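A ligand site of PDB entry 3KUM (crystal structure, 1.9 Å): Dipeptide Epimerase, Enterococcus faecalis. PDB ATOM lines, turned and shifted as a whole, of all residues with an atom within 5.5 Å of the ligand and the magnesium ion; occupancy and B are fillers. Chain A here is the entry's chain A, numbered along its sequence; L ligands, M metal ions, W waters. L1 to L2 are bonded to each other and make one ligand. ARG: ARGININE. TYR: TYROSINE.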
ATOM      1  N   PHE A  19      19.840   1.227  -5.994  1.00  0.00           N
ATOM      2  CA  PHE A  19      20.417   2.480  -6.476  1.00  0.00           C
ATOM      3  C   PHE A  19      19.595   3.678  -5.999  1.00  0.00           C
ATOM      4  O   PHE A  19      18.372   3.690  -6.111  1.00  0.00           O
ATOM      5  CB  PHE A  19      20.488   2.448  -8.006  1.00  0.00           C
ATOM      6  CG  PHE A  19      21.143   3.659  -8.612  1.00  0.00           C
ATOM      7  CD1 PHE A  19      22.461   3.999  -8.291  1.00  0.00           C
ATOM      8  CD2 PHE A  19      20.450   4.446  -9.533  1.00  0.00           C
ATOM      9  CE1 PHE A  19      23.078   5.109  -8.878  1.00  0.00           C
ATOM     10  CE2 PHE A  19      21.058   5.560 -10.122  1.00  0.00           C
ATOM     11  CZ  PHE A  19      22.371   5.892  -9.790  1.00  0.00           C
ATOM     12  N   ILE A  21      19.205   8.086  -5.895  1.00  0.00           N
ATOM     13  CA  ILE A  21      19.531   9.411  -6.399  1.00  0.00           C
ATOM     14  C   ILE A  21      18.572  10.392  -5.732  1.00  0.00           C
ATOM     15  O   ILE A  21      17.666   9.984  -5.003  1.00  0.00           O
ATOM     16  CB  ILE A  21      19.391   9.509  -7.948  1.00  0.00           C
ATOM     17  CG1 ILE A  21      17.914   9.411  -8.350  1.00  0.00           C
ATOM     18  CG2 ILE A  21      20.190   8.404  -8.617  1.00  0.00           C
ATOM     19  CD1 ILE A  21      17.678   9.711  -9.836  1.00  0.00           C
ATOM     20  N   ILE A  26      15.619   2.693  -6.662  1.00  0.00           N
ATOM     21  CA  ILE A  26      15.190   1.596  -7.526  1.00  0.00           C
ATOM     22  C   ILE A  26      15.972   0.335  -7.152  1.00  0.00           C
ATOM     23  O   ILE A  26      17.145   0.418  -6.810  1.00  0.00           O
ATOM     24  CB  ILE A  26      15.463   1.928  -9.022  1.00  0.00           C
ATOM     25  CG1 ILE A  26      15.127   0.717  -9.897  1.00  0.00           C
ATOM     26  CG2 ILE A  26      16.932   2.321  -9.201  1.00  0.00           C
ATOM     27  CD1 ILE A  26      15.459   0.923 -11.364  1.00  0.00           C
ATOM     28  N   GLY A  51      11.058   5.254 -16.583  1.00  0.00           N
ATOM     29  CA  GLY A  51      11.508   5.770 -15.294  1.00  0.00           C
ATOM     30  C   GLY A  51      10.445   6.695 -14.733  1.00  0.00           C
ATOM     31  O   GLY A  51      10.448   7.896 -15.044  1.00  0.00           O
ATOM     32  N   PHE A  53      10.012   8.338 -12.024  1.00  0.00           N
ATOM     33  CA  PHE A  53      10.421   9.625 -11.458  1.00  0.00           C
ATOM     34  C   PHE A  53      11.321  10.485 -12.340  1.00  0.00           C
ATOM     35  O   PHE A  53      11.827  11.506 -11.892  1.00  0.00           O
ATOM     36  CB  PHE A  53      11.044   9.456 -10.053  1.00  0.00           C
ATOM     37  CG  PHE A  53      12.210   8.525  -9.975  1.00  0.00           C
ATOM     38  CD1 PHE A  53      12.154   7.422  -9.134  1.00  0.00           C
ATOM     39  CD2 PHE A  53      13.379   8.771 -10.680  1.00  0.00           C
ATOM     40  CE1 PHE A  53      13.258   6.570  -8.991  1.00  0.00           C
ATOM     41  CE2 PHE A  53      14.490   7.938 -10.541  1.00  0.00           C
ATOM     42  CZ  PHE A  53      14.434   6.835  -9.700  1.00  0.00           C
ATOM     43  N   ILE A  54      11.497  10.083 -13.599  1.00  0.00           N
ATOM     44  CA  ILE A  54      12.296  10.860 -14.546  1.00  0.00           C
ATOM     45  C   ILE A  54      11.367  11.364 -15.661  1.00  0.00           C
ATOM     46  O   ILE A  54      11.283  12.564 -15.922  1.00  0.00           O
ATOM     47  CB  ILE A  54      13.399  10.004 -15.233  1.00  0.00           C
ATOM     48  CG1 ILE A  54      14.329   9.387 -14.195  1.00  0.00           C
ATOM     49  CG2 ILE A  54      14.187  10.891 -16.199  1.00  0.00           C
ATOM     50  CD1 ILE A  54      15.275  10.379 -13.534  1.00  0.00           C
ATOM     51  N   THR A 134      28.630   5.044 -12.381  1.00  0.00           N
ATOM     52  CA  THR A 134      27.997   5.897 -11.389  1.00  0.00           C
ATOM     53  C   THR A 134      28.072   5.330  -9.974  1.00  0.00           C
ATOM     54  O   THR A 134      28.231   4.122  -9.774  1.00  0.00           O
ATOM     55  CB  THR A 134      26.498   6.140 -11.752  1.00  0.00           C
ATOM     56  OG1 THR A 134      26.411   6.615 -13.104  1.00  0.00           O
ATOM     57  CG2 THR A 134      25.881   7.180 -10.834  1.00  0.00           C
ATOM     58  N   LYS A 159      30.902   8.948 -11.917  1.00  0.00           N
ATOM     59  CA  LYS A 159      29.761   9.851 -11.859  1.00  0.00           C
ATOM     60  C   LYS A 159      29.274   9.777 -10.415  1.00  0.00           C
ATOM     61  O   LYS A 159      28.987   8.700  -9.903  1.00  0.00           O
ATOM     62  CB  LYS A 159      28.655   9.398 -12.819  1.00  0.00           C
ATOM     63  CG  LYS A 159      27.434  10.309 -12.827  1.00  0.00           C
ATOM     64  CD  LYS A 159      26.500  10.032 -14.002  1.00  0.00           C
ATOM     65  CE  LYS A 159      25.325  10.993 -13.995  1.00  0.00           C
ATOM     66  NZ  LYS A 159      24.439  10.847 -15.184  1.00  0.00           N
ATOM     67  N   LYS A 161      26.512  10.957  -7.506  1.00  0.00           N
ATOM     68  CA  LYS A 161      25.198  11.516  -7.202  1.00  0.00           C
ATOM     69  C   LYS A 161      25.228  12.275  -5.887  1.00  0.00           C
ATOM     70  O   LYS A 161      25.897  11.884  -4.930  1.00  0.00           O
ATOM     71  CB  LYS A 161      24.152  10.399  -7.121  1.00  0.00           C
ATOM     72  CG  LYS A 161      23.869   9.681  -8.451  1.00  0.00           C
ATOM     73  CD  LYS A 161      23.038  10.562  -9.383  1.00  0.00           C
ATOM     74  CE  LYS A 161      22.726   9.838 -10.685  1.00  0.00           C
ATOM     75  NZ  LYS A 161      21.896  10.667 -11.604  1.00  0.00           N
ATOM     76  N   ASP A 189      26.243  14.786 -10.287  1.00  0.00           N
ATOM     77  CA  ASP A 189      24.858  14.828 -10.741  1.00  0.00           C
ATOM     78  C   ASP A 189      23.974  15.092  -9.517  1.00  0.00           C
ATOM     79  O   ASP A 189      23.876  14.240  -8.639  1.00  0.00           O
ATOM     80  CB  ASP A 189      24.471  13.497 -11.377  1.00  0.00           C
ATOM     81  CG  ASP A 189      23.181  13.572 -12.158  1.00  0.00           C
ATOM     82  OD1 ASP A 189      22.356  14.472 -11.879  1.00  0.00           O
ATOM     83  OD2 ASP A 189      22.972  12.723 -13.051  1.00  0.00           O
ATOM     84  N   ASN A 191      20.647  15.783  -9.716  1.00  0.00           N
ATOM     85  CA  ASN A 191      19.260  15.559 -10.085  1.00  0.00           C
ATOM     86  C   ASN A 191      18.269  16.619  -9.588  1.00  0.00           C
ATOM     87  O   ASN A 191      17.347  16.309  -8.832  1.00  0.00           O
ATOM     88  CB  ASN A 191      18.799  14.178  -9.639  1.00  0.00           C
ATOM     89  CG  ASN A 191      19.343  13.076 -10.521  1.00  0.00           C
ATOM     90  OD1 ASN A 191      20.282  12.362 -10.154  1.00  0.00           O
ATOM     91  ND2 ASN A 191      18.775  12.937 -11.720  1.00  0.00           N
ATOM     92  N   GLU A 215      25.976  18.022 -13.445  1.00  0.00           N
ATOM     93  CA  GLU A 215      24.760  17.688 -14.168  1.00  0.00           C
ATOM     94  C   GLU A 215      23.464  18.107 -13.476  1.00  0.00           C
ATOM     95  O   GLU A 215      23.260  17.844 -12.288  1.00  0.00           O
ATOM     96  CB  GLU A 215      24.736  16.163 -14.405  1.00  0.00           C
ATOM     97  CG  GLU A 215      23.674  15.649 -15.364  1.00  0.00           C
ATOM     98  CD  GLU A 215      23.878  14.179 -15.717  1.00  0.00           C
ATOM     99  OE1 GLU A 215      24.983  13.650 -15.475  1.00  0.00           O
ATOM    100  OE2 GLU A 215      22.933  13.559 -16.250  1.00  0.00           O
ATOM    101  N   GLN A 216      22.603  18.795 -14.230  1.00  0.00           N
ATOM    102  CA  GLN A 216      21.297  19.263 -13.759  1.00  0.00           C
ATOM    103  C   GLN A 216      21.237  19.672 -12.287  1.00  0.00           C
ATOM    104  O   GLN A 216      20.634  18.982 -11.458  1.00  0.00           O
ATOM    105  CB  GLN A 216      20.229  18.176 -14.019  1.00  0.00           C
ATOM    106  CG  GLN A 216      18.797  18.691 -14.023  1.00  0.00           C
ATOM    107  CD  GLN A 216      18.489  19.571 -15.224  1.00  0.00           C
ATOM    108  OE1 GLN A 216      18.864  19.238 -16.348  1.00  0.00           O
ATOM    109  NE2 GLN A 216      17.801  20.684 -14.988  1.00  0.00           N
ATOM    110  N   ASP A 240      20.216  17.636 -18.127  1.00  0.00           N
ATOM    111  CA  ASP A 240      19.736  16.281 -18.334  1.00  0.00           C
ATOM    112  C   ASP A 240      18.208  16.305 -18.419  1.00  0.00           C
ATOM    113  O   ASP A 240      17.651  16.320 -19.529  1.00  0.00           O
ATOM    114  CB  ASP A 240      20.206  15.357 -17.203  1.00  0.00           C
ATOM    115  CG  ASP A 240      19.736  13.913 -17.397  1.00  0.00           C
ATOM    116  OD1 ASP A 240      19.355  13.540 -18.534  1.00  0.00           O
ATOM    117  OD2 ASP A 240      19.772  13.139 -16.416  1.00  0.00           O
ATOM    118  N   GLU A 241      17.544  16.340 -17.275  1.00  0.00           N
ATOM    119  CA  GLU A 241      16.087  16.359 -17.246  1.00  0.00           C
ATOM    120  C   GLU A 241      15.477  17.585 -17.919  1.00  0.00           C
ATOM    121  O   GLU A 241      14.302  17.575 -18.279  1.00  0.00           O
ATOM    122  CB  GLU A 241      15.585  16.248 -15.794  1.00  0.00           C
ATOM    123  CG  GLU A 241      15.994  14.965 -15.083  1.00  0.00           C
ATOM    124  CD  GLU A 241      17.176  15.159 -14.133  1.00  0.00           C
ATOM    125  OE1 GLU A 241      18.231  15.650 -14.581  1.00  0.00           O
ATOM    126  OE2 GLU A 241      17.031  14.822 -12.930  1.00  0.00           O
ATOM    127  N   ASN A 262      23.029  16.012 -21.846  1.00  0.00           N
ATOM    128  CA  ASN A 262      22.961  14.558 -21.680  1.00  0.00           C
ATOM    129  C   ASN A 262      21.815  14.000 -22.526  1.00  0.00           C
ATOM    130  O   ASN A 262      20.662  14.431 -22.408  1.00  0.00           O
ATOM    131  CB  ASN A 262      22.716  14.201 -20.205  1.00  0.00           C
ATOM    132  CG  ASN A 262      22.558  12.705 -19.990  1.00  0.00           C
ATOM    133  OD1 ASN A 262      21.806  12.034 -20.691  1.00  0.00           O
ATOM    134  ND2 ASN A 262      23.254  12.171 -18.984  1.00  0.00           N
ATOM    135  N   LYS A 264      19.545  10.677 -23.712  1.00  0.00           N
ATOM    136  CA  LYS A 264      19.109   9.344 -23.306  1.00  0.00           C
ATOM    137  C   LYS A 264      18.057   8.894 -24.310  1.00  0.00           C
ATOM    138  O   LYS A 264      17.101   9.622 -24.579  1.00  0.00           O
ATOM    139  CB  LYS A 264      18.484   9.348 -21.899  1.00  0.00           C
ATOM    140  CG  LYS A 264      19.463   9.464 -20.741  1.00  0.00           C
ATOM    141  CD  LYS A 264      18.717   9.346 -19.415  1.00  0.00           C
ATOM    142  CE  LYS A 264      19.618   9.576 -18.212  1.00  0.00           C
ATOM    143  NZ  LYS A 264      20.115  10.971 -18.169  1.00  0.00           N
ATOM    144  N   CYS A 292      21.839   6.839 -19.522  1.00  0.00           N
ATOM    145  CA  CYS A 292      20.935   5.703 -19.478  1.00  0.00           C
ATOM    146  C   CYS A 292      20.058   5.738 -18.250  1.00  0.00           C
ATOM    147  O   CYS A 292      20.355   6.446 -17.289  1.00  0.00           O
ATOM    148  CB  CYS A 292      21.719   4.379 -19.494  1.00  0.00           C
ATOM    149  SG  CYS A 292      22.776   4.098 -18.032  1.00  0.00           S
ATOM    150  N   MET A 293      18.974   4.971 -18.289  1.00  0.00           N
ATOM    151  CA  MET A 293      18.035   4.877 -17.173  1.00  0.00           C
ATOM    152  C   MET A 293      18.481   3.674 -16.362  1.00  0.00           C
ATOM    153  O   MET A 293      19.112   2.767 -16.895  1.00  0.00           O
ATOM    154  CB  MET A 293      16.608   4.630 -17.687  1.00  0.00           C
ATOM    155  CG  MET A 293      16.087   5.668 -18.656  1.00  0.00           C
ATOM    156  SD  MET A 293      15.828   7.232 -17.866  1.00  0.00           S
ATOM    157  CE  MET A 293      14.042   7.242 -17.683  1.00  0.00           C
ATOM    158  N   ALA A 294      18.148   3.663 -15.077  1.00  0.00           N
ATOM    159  CA  ALA A 294      18.504   2.533 -14.234  1.00  0.00           C
ATOM    160  C   ALA A 294      17.688   1.303 -14.632  1.00  0.00           C
ATOM    161  O   ALA A 294      18.149   0.170 -14.460  1.00  0.00           O
ATOM    162  CB  ALA A 294      18.240   2.878 -12.766  1.00  0.00           C
ATOM    163  N   GLU A 295      16.499   1.531 -15.198  1.00  0.00           N
ATOM    164  CA  GLU A 295      15.617   0.441 -15.618  1.00  0.00           C
ATOM    165  C   GLU A 295      15.871  -0.186 -16.989  1.00  0.00           C
ATOM    166  O   GLU A 295      15.151  -1.105 -17.387  1.00  0.00           O
ATOM    167  CB  GLU A 295      14.153   0.903 -15.562  1.00  0.00           C
ATOM    168  CG  GLU A 295      13.720   1.431 -14.214  1.00  0.00           C
ATOM    169  CD  GLU A 295      13.623   2.941 -14.188  1.00  0.00           C
ATOM    170  OE1 GLU A 295      14.511   3.610 -14.775  1.00  0.00           O
ATOM    171  OE2 GLU A 295      12.662   3.467 -13.578  1.00  0.00           O
ATOM    172  N   ASP A 318      27.900   7.533 -20.272  1.00  0.00           N
ATOM    173  CA  ASP A 318      27.468   7.066 -18.953  1.00  0.00           C
ATOM    174  C   ASP A 318      26.527   5.896 -19.228  1.00  0.00           C
ATOM    175  O   ASP A 318      25.315   5.999 -19.059  1.00  0.00           O
ATOM    176  CB  ASP A 318      26.745   8.190 -18.205  1.00  0.00           C
ATOM    177  CG  ASP A 318      26.183   7.733 -16.865  1.00  0.00           C
ATOM    178  OD1 ASP A 318      26.803   6.866 -16.225  1.00  0.00           O
ATOM    179  OD2 ASP A 318      25.127   8.272 -16.438  1.00  0.00           O
ATOM    180  N   ASP A 320      26.317   2.527 -17.860  1.00  0.00           N
ATOM    181  CA  ASP A 320      26.652   1.561 -16.821  1.00  0.00           C
ATOM    182  C   ASP A 320      25.470   0.756 -16.283  1.00  0.00           C
ATOM    183  O   ASP A 320      25.580   0.118 -15.231  1.00  0.00           O
ATOM    184  CB  ASP A 320      27.303   2.304 -15.653  1.00  0.00           C
ATOM    185  CG  ASP A 320      26.389   3.361 -15.071  1.00  0.00           C
ATOM    186  OD1 ASP A 320      25.413   3.758 -15.751  1.00  0.00           O
ATOM    187  OD2 ASP A 320      26.647   3.812 -13.940  1.00  0.00           O
ATOM    188  N   ALA A 321      24.352   0.777 -16.996  1.00  0.00           N
ATOM    189  CA  ALA A 321      23.170   0.042 -16.548  1.00  0.00           C
ATOM    190  C   ALA A 321      23.407  -1.474 -16.438  1.00  0.00           C
ATOM    191  O   ALA A 321      22.936  -2.117 -15.498  1.00  0.00           O
ATOM    192  CB  ALA A 321      21.997   0.324 -17.487  1.00  0.00           C
ATOM    193  N   PHE A 323      26.061  -3.091 -15.653  1.00  0.00           N
ATOM    194  CA  PHE A 323      26.977  -3.466 -14.572  1.00  0.00           C
ATOM    195  C   PHE A 323      26.264  -3.865 -13.288  1.00  0.00           C
ATOM    196  O   PHE A 323      26.812  -4.605 -12.471  1.00  0.00           O
ATOM    197  CB  PHE A 323      27.933  -2.312 -14.239  1.00  0.00           C
ATOM    198  CG  PHE A 323      28.678  -1.754 -15.422  1.00  0.00           C
ATOM    199  CD1 PHE A 323      28.927  -2.550 -16.545  1.00  0.00           C
ATOM    200  CD2 PHE A 323      29.161  -0.446 -15.401  1.00  0.00           C
ATOM    201  CE1 PHE A 323      29.641  -2.048 -17.625  1.00  0.00           C
ATOM    202  CE2 PHE A 323      29.870   0.068 -16.485  1.00  0.00           C
ATOM    203  CZ  PHE A 323      30.115  -0.737 -17.606  1.00  0.00           C
ATOM    204  N   GLY A 324      25.042  -3.375 -13.111  1.00  0.00           N
ATOM    205  CA  GLY A 324      24.287  -3.698 -11.914  1.00  0.00           C
ATOM    206  C   GLY A 324      23.269  -4.814 -12.056  1.00  0.00           C
ATOM    207  O   GLY A 324      22.619  -5.163 -11.077  1.00  0.00           O
HETATM  208  N   ARG L   1      23.922   6.388 -14.687  1.00  0.00           N
HETATM  209  CA  ARG L   1      22.434   6.229 -14.743  1.00  0.00           C
HETATM  210  C   ARG L   1      21.754   7.510 -14.287  1.00  0.00           C
HETATM  211  O   ARG L   1      22.279   8.239 -13.445  1.00  0.00           O
HETATM  212  CB  ARG L   1      21.993   5.078 -13.841  1.00  0.00           C
HETATM  213  CG  ARG L   1      22.826   3.836 -13.953  1.00  0.00           C
HETATM  214  CD  ARG L   1      22.650   2.997 -12.705  1.00  0.00           C
HETATM  215  NE  ARG L   1      23.734   2.038 -12.539  1.00  0.00           N
HETATM  216  CZ  ARG L   1      23.998   1.401 -11.402  1.00  0.00           C
HETATM  217  NH1 ARG L   1      23.243   1.631 -10.328  1.00  0.00           N
HETATM  218  NH2 ARG L   1      24.997   0.543 -11.335  1.00  0.00           N
HETATM  219  N   TYR L   2      20.573   7.771 -14.838  1.00  0.00           N
HETATM  220  CA  TYR L   2      19.807   8.956 -14.484  1.00  0.00           C
HETATM  221  C   TYR L   2      20.613  10.251 -14.571  1.00  0.00           C
HETATM  222  O   TYR L   2      21.653  10.257 -15.257  1.00  0.00           O
HETATM  223  CB  TYR L   2      19.242   8.799 -13.062  1.00  0.00           C
HETATM  224  CG  TYR L   2      18.254   7.671 -12.917  1.00  0.00           C
HETATM  225  CD1 TYR L   2      18.240   6.893 -11.765  1.00  0.00           C
HETATM  226  CD2 TYR L   2      17.332   7.376 -13.930  1.00  0.00           C
HETATM  227  CE1 TYR L   2      17.343   5.853 -11.608  1.00  0.00           C
HETATM  228  CE2 TYR L   2      16.424   6.327 -13.783  1.00  0.00           C
HETATM  229  CZ  TYR L   2      16.437   5.573 -12.623  1.00  0.00           C
HETATM  230  OH  TYR L   2      15.574   4.510 -12.456  1.00  0.00           O
HETATM  231  OXT TYR L   2      20.149  11.248 -13.973  1.00  0.00           O
HETATM  232 MG    MG M   1      21.529  13.105 -14.759  1.00  0.00          MG
HETATM  233  O   HOH W   1      21.850  -0.321 -11.225  1.00  0.00           O
HETATM  234  O   HOH W   2      22.821   9.110 -17.650  1.00  0.00           O
HETATM  235  O   HOH W   3      17.530  11.441 -16.070  1.00  0.00           O
HETATM  236  O   HOH W   4      20.592  14.742 -13.916  1.00  0.00           O
HETATM  237  O   HOH W   5      26.984  -0.990 -10.820  1.00  0.00           O
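Water W4 lies within hydrogen-bond range of OE1 of Glu 241 (2.6 Å), OD1 of Asp 189 (2.7 Å) and ND2 of Asn 191 (3.4 Å).
Residues that only touch the magnesium ion: Lys 159.
An oxygen (OH) of TYR L2 is in hydrogen-bond range of the side-chain carboxylate of Glu 295 (2.7 Å). The backbone carbonyl oxygen (O) of Cys 292 is in hydrogen-bond range of a nitrogen (N) of TYR L2, at 2.8 Å. OD2 of Asp 318 lies within salt-bridge range of N of ARG L1 (2.8 Å). The side-chain amino group of Lys 159 is in salt-bridge range of an oxygen (O) of TYR L2, at 2.8 Å. The side-chain hydroxyl (OG1) of Thr 134 lies within hydrogen-bond range of a nitrogen (N) of ARG L1, 3.0 Å away. The side-chain amino group (NZ) of Lys 161 lies within salt-bridge range of an oxygen (O) of TYR L2, at 3.7 Å. An oxygen (OXT) of TYR L2 lies close to the side-chain amide nitrogen of Asn 191 (3.1 Å). OD1 of Asp 320 is in salt-bridge range of N of ARG L1, 3.2 Å away. NZ of Lys 264 lies within salt-bridge range of O of TYR L2, 3.4 Å away.
The magnesium ion is bound by water W4, the side-chain carboxylate of Glu 215, the side-chain carboxylate of Asp 189, the side-chain carboxylate of Asp 240 and an oxygen (OXT) of TYR L2. The magnesium ion has five donor atoms within binding distance.
CD1 of Phe 19 touches NH1 of ARG L1 (3.2 Å). Ile 21 touches the ligand. Ile 26 touches the ligand. CZ of Phe 53 touches CE1 of TYR L2, at 3.6 Å. CG1 of Ile 54 touches CD2 of TYR L2, at 3.6 Å. Ala 294 touches the ligand. Of the 26 residues printed, 18 come within 4 Å of the ligand.
The side-chain carboxylate of Glu 215 lies within salt-bridge range of the side-chain amino group of Lys 159. The side-chain carboxylate of Asp 189 sits close to the side-chain amino group of Lys 159. The side-chain carboxylate (OD1) of Asp 189 lies within salt-bridge range of the side-chain amino group (NZ) of Lys 161, 3.8 Å away. The side-chain carboxylate (OD1) of Asp 189 is in hydrogen-bond range of the backbone NH (N) of Asn 191. The backbone NH (N) of Asp 240 sits at hydrogen-bond distance from the side-chain amide oxygen (OE1) of Gln 216, at 2.7 Å. The side-chain sulfur of Cys 292 sits at hydrogen-bond distance from the backbone carbonyl oxygen of Asp 318. OD1 of Asp 318 sits at hydrogen-bond distance from OG1 of Thr 134 (3.2 Å). O of Ile 26 is in hydrogen-bond range of N of Phe 19 (2.9 Å).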
